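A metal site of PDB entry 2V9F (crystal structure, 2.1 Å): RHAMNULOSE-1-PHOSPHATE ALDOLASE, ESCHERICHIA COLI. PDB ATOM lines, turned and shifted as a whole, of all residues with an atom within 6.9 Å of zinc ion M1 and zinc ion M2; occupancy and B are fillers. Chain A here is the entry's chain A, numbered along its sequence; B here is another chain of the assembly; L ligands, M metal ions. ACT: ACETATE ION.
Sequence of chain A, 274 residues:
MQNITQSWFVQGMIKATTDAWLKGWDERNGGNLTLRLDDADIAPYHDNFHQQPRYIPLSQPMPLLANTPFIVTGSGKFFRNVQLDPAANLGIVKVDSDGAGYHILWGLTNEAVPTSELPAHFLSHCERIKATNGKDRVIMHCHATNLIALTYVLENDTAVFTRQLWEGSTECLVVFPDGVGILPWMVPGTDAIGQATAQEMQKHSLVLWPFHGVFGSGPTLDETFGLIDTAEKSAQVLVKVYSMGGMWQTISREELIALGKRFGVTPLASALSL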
ATOM      1  N   TRP A  25      23.221  18.741  -5.501  1.00  0.00           N
ATOM      2  CA  TRP A  25      23.354  18.221  -4.154  1.00  0.00           C
ATOM      3  C   TRP A  25      24.391  18.951  -3.314  1.00  0.00           C
ATOM      4  O   TRP A  25      24.378  18.837  -2.084  1.00  0.00           O
ATOM      5  CB  TRP A  25      23.808  16.758  -4.173  1.00  0.00           C
ATOM      6  CG  TRP A  25      22.911  15.784  -4.860  1.00  0.00           C
ATOM      7  CD1 TRP A  25      21.595  15.953  -5.175  1.00  0.00           C
ATOM      8  CD2 TRP A  25      23.261  14.465  -5.277  1.00  0.00           C
ATOM      9  NE1 TRP A  25      21.105  14.804  -5.752  1.00  0.00           N
ATOM     10  CE2 TRP A  25      22.110  13.873  -5.823  1.00  0.00           C
ATOM     11  CE3 TRP A  25      24.452  13.717  -5.231  1.00  0.00           C
ATOM     12  CZ2 TRP A  25      22.105  12.575  -6.333  1.00  0.00           C
ATOM     13  CZ3 TRP A  25      24.453  12.421  -5.733  1.00  0.00           C
ATOM     14  CH2 TRP A  25      23.278  11.867  -6.276  1.00  0.00           C
ATOM     15  N   ASP A  26      25.303  19.662  -3.967  1.00  0.00           N
ATOM     16  CA  ASP A  26      26.363  20.312  -3.225  1.00  0.00           C
ATOM     17  C   ASP A  26      26.568  21.784  -3.495  1.00  0.00           C
ATOM     18  O   ASP A  26      27.527  22.181  -4.146  1.00  0.00           O
ATOM     19  CB  ASP A  26      27.673  19.564  -3.459  1.00  0.00           C
ATOM     20  CG  ASP A  26      27.569  18.087  -3.104  1.00  0.00           C
ATOM     21  OD1 ASP A  26      26.881  17.340  -3.824  1.00  0.00           O
ATOM     22  OD2 ASP A  26      28.177  17.680  -2.088  1.00  0.00           O
ATOM     23  N   GLU A  27      25.651  22.594  -3.010  1.00  0.00           N
ATOM     24  CA  GLU A  27      25.769  24.022  -3.176  1.00  0.00           C
ATOM     25  C   GLU A  27      26.837  24.486  -2.206  1.00  0.00           C
ATOM     26  O   GLU A  27      27.062  23.865  -1.152  1.00  0.00           O
ATOM     27  CB  GLU A  27      24.441  24.727  -2.842  1.00  0.00           C
ATOM     28  CG  GLU A  27      23.929  24.415  -1.457  1.00  0.00           C
ATOM     29  CD  GLU A  27      23.439  22.988  -1.319  1.00  0.00           C
ATOM     30  OE1 GLU A  27      23.184  22.560  -0.190  1.00  0.00           O
ATOM     31  OE2 GLU A  27      23.290  22.267  -2.345  1.00  0.00           O
ATOM     32  N   ARG A  28      27.501  25.580  -2.575  1.00  0.00           N
ATOM     33  CA  ARG A  28      28.526  26.171  -1.743  1.00  0.00           C
ATOM     34  C   ARG A  28      29.499  25.097  -1.308  1.00  0.00           C
ATOM     35  O   ARG A  28      30.069  24.397  -2.150  1.00  0.00           O
ATOM     36  CB  ARG A  28      27.873  26.825  -0.528  1.00  0.00           C
ATOM     37  CG  ARG A  28      28.781  27.776   0.233  1.00  0.00           C
ATOM     38  CD  ARG A  28      27.991  28.570   1.254  1.00  0.00           C
ATOM     39  NE  ARG A  28      28.831  29.592   1.875  1.00  0.00           N
ATOM     40  CZ  ARG A  28      29.798  29.332   2.755  1.00  0.00           C
ATOM     41  NH1 ARG A  28      30.044  28.088   3.134  1.00  0.00           N
ATOM     42  NH2 ARG A  28      30.535  30.324   3.229  1.00  0.00           N
ATOM     43  N   ASN A  29      29.669  24.950   0.003  1.00  0.00           N
ATOM     44  CA  ASN A  29      30.591  23.972   0.586  1.00  0.00           C
ATOM     45  C   ASN A  29      29.798  22.826   1.197  1.00  0.00           C
ATOM     46  O   ASN A  29      30.338  22.036   1.991  1.00  0.00           O
ATOM     47  CB  ASN A  29      31.412  24.628   1.681  1.00  0.00           C
ATOM     48  CG  ASN A  29      30.550  25.052   2.869  1.00  0.00           C
ATOM     49  OD1 ASN A  29      29.486  25.649   2.696  1.00  0.00           O
ATOM     50  ND2 ASN A  29      30.995  24.723   4.082  1.00  0.00           N
ATOM     51  N   GLY A  30      28.512  22.745   0.860  1.00  0.00           N
ATOM     52  CA  GLY A  30      27.680  21.680   1.396  1.00  0.00           C
ATOM     53  C   GLY A  30      28.082  20.356   0.778  1.00  0.00           C
ATOM     54  O   GLY A  30      27.944  20.158  -0.427  1.00  0.00           O
ATOM     55  N   GLY A  31      28.587  19.438   1.585  1.00  0.00           N
ATOM     56  CA  GLY A  31      28.985  18.144   1.057  1.00  0.00           C
ATOM     57  C   GLY A  31      30.476  17.862   1.192  1.00  0.00           C
ATOM     58  O   GLY A  31      31.303  18.787   1.242  1.00  0.00           O
ATOM     59  N   ASN A  32      30.824  16.588   1.262  1.00  0.00           N
ATOM     60  CA  ASN A  32      32.223  16.203   1.377  1.00  0.00           C
ATOM     61  C   ASN A  32      32.431  14.747   0.971  1.00  0.00           C
ATOM     62  O   ASN A  32      31.518  13.922   1.015  1.00  0.00           O
ATOM     63  CB  ASN A  32      32.726  16.473   2.809  1.00  0.00           C
ATOM     64  CG  ASN A  32      31.604  16.614   3.812  1.00  0.00           C
ATOM     65  OD1 ASN A  32      31.080  15.626   4.315  1.00  0.00           O
ATOM     66  ND2 ASN A  32      31.208  17.865   4.097  1.00  0.00           N
ATOM     67  N   GLU A 117      33.903  17.841   8.482  1.00  0.00           N
ATOM     68  CA  GLU A 117      33.122  16.633   8.753  1.00  0.00           C
ATOM     69  C   GLU A 117      34.010  15.401   8.780  1.00  0.00           C
ATOM     70  O   GLU A 117      33.512  14.267   8.790  1.00  0.00           O
ATOM     71  CB  GLU A 117      32.012  16.444   7.695  1.00  0.00           C
ATOM     72  CG  GLU A 117      30.879  17.460   7.830  1.00  0.00           C
ATOM     73  CD  GLU A 117      30.286  17.492   9.236  1.00  0.00           C
ATOM     74  OE1 GLU A 117      29.606  18.484   9.563  1.00  0.00           O
ATOM     75  OE2 GLU A 117      30.495  16.538  10.020  1.00  0.00           O
ATOM     76  N   HIS A 141      29.242  12.393   1.486  1.00  0.00           N
ATOM     77  CA  HIS A 141      28.197  13.174   2.084  1.00  0.00           C
ATOM     78  C   HIS A 141      27.701  14.219   1.093  1.00  0.00           C
ATOM     79  O   HIS A 141      28.487  14.927   0.483  1.00  0.00           O
ATOM     80  CB  HIS A 141      28.707  13.875   3.344  1.00  0.00           C
ATOM     81  CG  HIS A 141      27.734  14.851   3.918  1.00  0.00           C
ATOM     82  ND1 HIS A 141      26.442  14.506   4.270  1.00  0.00           N
ATOM     83  CD2 HIS A 141      27.859  16.166   4.226  1.00  0.00           C
ATOM     84  CE1 HIS A 141      25.819  15.563   4.747  1.00  0.00           C
ATOM     85  NE2 HIS A 141      26.662  16.579   4.733  1.00  0.00           N
ATOM     86  N   CYS A 142      26.393  14.314   0.956  1.00  0.00           N
ATOM     87  CA  CYS A 142      25.844  15.294   0.045  1.00  0.00           C
ATOM     88  C   CYS A 142      24.485  15.717   0.539  1.00  0.00           C
ATOM     89  O   CYS A 142      23.831  15.003   1.301  1.00  0.00           O
ATOM     90  CB  CYS A 142      25.756  14.728  -1.363  1.00  0.00           C
ATOM     91  SG  CYS A 142      24.408  13.604  -1.575  1.00  0.00           S
ATOM     92  N   HIS A 143      24.082  16.904   0.116  1.00  0.00           N
ATOM     93  CA  HIS A 143      22.800  17.443   0.513  1.00  0.00           C
ATOM     94  C   HIS A 143      21.756  17.153  -0.540  1.00  0.00           C
ATOM     95  O   HIS A 143      21.306  18.051  -1.242  1.00  0.00           O
ATOM     96  CB  HIS A 143      22.950  18.937   0.758  1.00  0.00           C
ATOM     97  CG  HIS A 143      23.930  19.255   1.842  1.00  0.00           C
ATOM     98  ND1 HIS A 143      24.176  20.545   2.266  1.00  0.00           N
ATOM     99  CD2 HIS A 143      24.720  18.455   2.582  1.00  0.00           C
ATOM    100  CE1 HIS A 143      25.089  20.521   3.224  1.00  0.00           C
ATOM    101  NE2 HIS A 143      25.442  19.258   3.434  1.00  0.00           N
ATOM    102  N   ILE A 148      16.370  15.233   1.973  1.00  0.00           N
ATOM    103  CA  ILE A 148      16.288  16.257   3.006  1.00  0.00           C
ATOM    104  C   ILE A 148      14.823  16.647   3.198  1.00  0.00           C
ATOM    105  O   ILE A 148      14.313  16.609   4.320  1.00  0.00           O
ATOM    106  CB  ILE A 148      17.129  17.511   2.609  1.00  0.00           C
ATOM    107  CG1 ILE A 148      18.625  17.156   2.692  1.00  0.00           C
ATOM    108  CG2 ILE A 148      16.799  18.688   3.538  1.00  0.00           C
ATOM    109  CD1 ILE A 148      19.553  18.161   2.043  1.00  0.00           C
ATOM    110  N   PRO A 188      26.497  19.543  13.411  1.00  0.00           N
ATOM    111  CA  PRO A 188      27.453  18.968  12.458  1.00  0.00           C
ATOM    112  C   PRO A 188      28.894  19.356  12.794  1.00  0.00           C
ATOM    113  O   PRO A 188      29.122  20.294  13.565  1.00  0.00           O
ATOM    114  CB  PRO A 188      26.976  19.533  11.114  1.00  0.00           C
ATOM    115  CG  PRO A 188      26.448  20.887  11.496  1.00  0.00           C
ATOM    116  CD  PRO A 188      25.702  20.617  12.792  1.00  0.00           C
ATOM    117  N   TRP A 209      20.990  12.542   7.951  1.00  0.00           N
ATOM    118  CA  TRP A 209      21.119  13.550   8.980  1.00  0.00           C
ATOM    119  C   TRP A 209      19.876  14.401   8.688  1.00  0.00           C
ATOM    120  O   TRP A 209      19.854  15.159   7.719  1.00  0.00           O
ATOM    121  CB  TRP A 209      22.386  14.362   8.783  1.00  0.00           C
ATOM    122  CG  TRP A 209      23.633  13.662   9.146  1.00  0.00           C
ATOM    123  CD1 TRP A 209      23.770  12.380   9.630  1.00  0.00           C
ATOM    124  CD2 TRP A 209      24.947  14.241   9.180  1.00  0.00           C
ATOM    125  NE1 TRP A 209      25.081  12.144   9.971  1.00  0.00           N
ATOM    126  CE2 TRP A 209      25.821  13.264   9.706  1.00  0.00           C
ATOM    127  CE3 TRP A 209      25.459  15.509   8.824  1.00  0.00           C
ATOM    128  CZ2 TRP A 209      27.192  13.512   9.887  1.00  0.00           C
ATOM    129  CZ3 TRP A 209      26.826  15.745   8.998  1.00  0.00           C
ATOM    130  CH2 TRP A 209      27.675  14.751   9.521  1.00  0.00           C
ATOM    131  N   HIS A 212      19.467  18.029   7.001  1.00  0.00           N
ATOM    132  CA  HIS A 212      20.832  18.331   6.630  1.00  0.00           C
ATOM    133  C   HIS A 212      21.254  17.594   5.366  1.00  0.00           C
ATOM    134  O   HIS A 212      21.521  18.235   4.342  1.00  0.00           O
ATOM    135  CB  HIS A 212      21.755  17.989   7.832  1.00  0.00           C
ATOM    136  CG  HIS A 212      23.182  18.389   7.623  1.00  0.00           C
ATOM    137  ND1 HIS A 212      24.024  18.696   8.674  1.00  0.00           N
ATOM    138  CD2 HIS A 212      23.913  18.528   6.502  1.00  0.00           C
ATOM    139  CE1 HIS A 212      25.216  19.007   8.200  1.00  0.00           C
ATOM    140  NE2 HIS A 212      25.173  18.916   6.889  1.00  0.00           N
ATOM    141  N   GLY A 213      21.303  16.261   5.408  1.00  0.00           N
ATOM    142  CA  GLY A 213      21.731  15.524   4.226  1.00  0.00           C
ATOM    143  C   GLY A 213      21.871  14.035   4.385  1.00  0.00           C
ATOM    144  O   GLY A 213      21.221  13.424   5.233  1.00  0.00           O
ATOM    145  N   VAL A 214      22.752  13.437   3.573  1.00  0.00           N
ATOM    146  CA  VAL A 214      22.946  11.986   3.576  1.00  0.00           C
ATOM    147  C   VAL A 214      24.420  11.588   3.528  1.00  0.00           C
ATOM    148  O   VAL A 214      25.259  12.307   2.967  1.00  0.00           O
ATOM    149  CB  VAL A 214      22.182  11.363   2.349  1.00  0.00           C
ATOM    150  CG1 VAL A 214      22.849  11.763   1.047  1.00  0.00           C
ATOM    151  CG2 VAL A 214      22.133   9.850   2.451  1.00  0.00           C
ATOM    152  N   PHE A 215      24.727  10.448   4.141  1.00  0.00           N
ATOM    153  CA  PHE A 215      26.077   9.869   4.167  1.00  0.00           C
ATOM    154  C   PHE A 215      25.959   8.485   3.548  1.00  0.00           C
ATOM    155  O   PHE A 215      25.025   7.744   3.845  1.00  0.00           O
ATOM    156  CB  PHE A 215      26.612   9.720   5.608  1.00  0.00           C
ATOM    157  CG  PHE A 215      27.462  10.862   6.061  1.00  0.00           C
ATOM    158  CD1 PHE A 215      26.893  12.082   6.390  1.00  0.00           C
ATOM    159  CD2 PHE A 215      28.849  10.738   6.098  1.00  0.00           C
ATOM    160  CE1 PHE A 215      27.695  13.163   6.746  1.00  0.00           C
ATOM    161  CE2 PHE A 215      29.660  11.819   6.449  1.00  0.00           C
ATOM    162  CZ  PHE A 215      29.078  13.037   6.774  1.00  0.00           C
ATOM    163  N   SER B 169      17.621  23.924   5.749  1.00  0.00           N
ATOM    164  CA  SER B 169      18.950  23.341   5.497  1.00  0.00           C
ATOM    165  C   SER B 169      19.793  23.741   6.688  1.00  0.00           C
ATOM    166  O   SER B 169      19.897  24.933   7.013  1.00  0.00           O
ATOM    167  CB  SER B 169      19.578  23.880   4.198  1.00  0.00           C
ATOM    168  OG  SER B 169      19.013  23.255   3.043  1.00  0.00           O
ATOM    169  N   THR B 170      20.380  22.756   7.358  1.00  0.00           N
ATOM    170  CA  THR B 170      21.177  23.016   8.562  1.00  0.00           C
ATOM    171  C   THR B 170      22.257  24.100   8.477  1.00  0.00           C
ATOM    172  O   THR B 170      22.370  24.932   9.378  1.00  0.00           O
ATOM    173  CB  THR B 170      21.848  21.707   9.066  1.00  0.00           C
ATOM    174  OG1 THR B 170      20.833  20.826   9.545  1.00  0.00           O
ATOM    175  CG2 THR B 170      22.872  21.981  10.198  1.00  0.00           C
ATOM    176  N   GLU B 171      23.035  24.112   7.404  1.00  0.00           N
ATOM    177  CA  GLU B 171      24.106  25.103   7.282  1.00  0.00           C
ATOM    178  C   GLU B 171      23.649  26.549   7.088  1.00  0.00           C
ATOM    179  O   GLU B 171      24.470  27.462   7.183  1.00  0.00           O
ATOM    180  CB  GLU B 171      25.014  24.754   6.114  1.00  0.00           C
ATOM    181  CG  GLU B 171      24.427  25.158   4.793  1.00  0.00           C
ATOM    182  CD  GLU B 171      23.718  24.018   4.093  1.00  0.00           C
ATOM    183  OE1 GLU B 171      23.181  23.096   4.766  1.00  0.00           O
ATOM    184  OE2 GLU B 171      23.671  24.069   2.859  1.00  0.00           O
ATOM    185  N   CYS B 172      22.375  26.763   6.805  1.00  0.00           N
ATOM    186  CA  CYS B 172      21.885  28.118   6.552  1.00  0.00           C
ATOM    187  C   CYS B 172      22.180  29.127   7.637  1.00  0.00           C
ATOM    188  O   CYS B 172      22.659  30.238   7.353  1.00  0.00           O
ATOM    189  CB  CYS B 172      20.388  28.099   6.239  1.00  0.00           C
ATOM    190  SG  CYS B 172      20.058  27.434   4.574  1.00  0.00           S
ATOM    191  N   THR B 230      22.825  28.648  -1.362  1.00  0.00           N
ATOM    192  CA  THR B 230      22.467  28.001  -0.109  1.00  0.00           C
ATOM    193  C   THR B 230      21.037  28.386   0.271  1.00  0.00           C
ATOM    194  O   THR B 230      20.241  27.540   0.688  1.00  0.00           O
ATOM    195  CB  THR B 230      23.459  28.392   1.017  1.00  0.00           C
ATOM    196  OG1 THR B 230      24.762  27.893   0.692  1.00  0.00           O
ATOM    197  CG2 THR B 230      23.023  27.813   2.357  1.00  0.00           C
ATOM    198  N   LYS B 233      18.682  26.733  -2.148  1.00  0.00           N
ATOM    199  CA  LYS B 233      18.635  25.297  -1.890  1.00  0.00           C
ATOM    200  C   LYS B 233      17.647  25.034  -0.752  1.00  0.00           C
ATOM    201  O   LYS B 233      16.814  24.123  -0.828  1.00  0.00           O
ATOM    202  CB  LYS B 233      20.018  24.760  -1.507  1.00  0.00           C
ATOM    203  CG  LYS B 233      20.038  23.366  -0.877  1.00  0.00           C
ATOM    204  CD  LYS B 233      19.311  22.337  -1.712  1.00  0.00           C
ATOM    205  CE  LYS B 233      19.782  20.909  -1.399  1.00  0.00           C
ATOM    206  NZ  LYS B 233      21.082  20.608  -2.093  1.00  0.00           N
ATOM    207  N   SER B 234      17.733  25.852   0.293  1.00  0.00           N
ATOM    208  CA  SER B 234      16.826  25.703   1.417  1.00  0.00           C
ATOM    209  C   SER B 234      15.412  26.004   0.935  1.00  0.00           C
ATOM    210  O   SER B 234      14.475  25.295   1.285  1.00  0.00           O
ATOM    211  CB  SER B 234      17.219  26.648   2.560  1.00  0.00           C
ATOM    212  OG  SER B 234      16.327  26.496   3.651  1.00  0.00           O
HETATM  213  C   ACT L   1      28.704  20.163   5.280  1.00  0.00           C
HETATM  214  O   ACT L   1      27.601  20.684   5.548  1.00  0.00           O
HETATM  215  OXT ACT L   1      28.830  18.999   4.853  1.00  0.00           O
HETATM  216  CH3 ACT L   1      29.966  20.995   5.508  1.00  0.00           C
HETATM  217 ZN    ZN M   1      26.504  18.710   5.143  1.00  0.00          ZN
HETATM  218 ZN    ZN M   2      23.225  22.323   1.756  1.00  0.00          ZN
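Three residues have an atom within 4 Å of zinc ion M1: His 141, His 143 and His 212.
The side-chain carboxylate of Glu 27 is in salt-bridge range of the side-chain amino group of Lys 233 of chain B (2.8 Å). NZ of Lys 233 of chain B is in hydrogen-bond range of O of His 143, at 2.7 Å. N of His 143 lies within hydrogen-bond range of O of Trp 25 (2.9 Å). The backbone NH (N) of His 141 sits at hydrogen-bond distance from the backbone carbonyl oxygen (O) of Asn 32 (2.8 Å). The backbone carbonyl oxygen of Val 214 sits at hydrogen-bond distance from a ring nitrogen (ND1) of His 141, at 2.8 Å.
Zinc ion M2 is bound by the side-chain carboxylate (OE1) of Glu 27 (2.0 Å), a ring nitrogen (ND1) of His 143 (2.1 Å) and the side-chain carboxylate (OE2) of Glu 171 of chain B (2.1 Å).
Three residues have an atom within 4 Å of zinc ion M2: Glu 27, His 143 and Glu 171 of chain B. The nearest printed residue that does not touch zinc ion M2 is Lys 233 of chain B (4.3 Å).
Zinc ion M1 is bound by a ring nitrogen (NE2) of His 143 (2.1 Å), a ring nitrogen (NE2) of His 141 (2.2 Å), a ring nitrogen (NE2) of His 212 (2.2 Å), an oxygen (O) of the ligand (2.3 Å) and an oxygen (OXT) of the ligand (2.4 Å).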
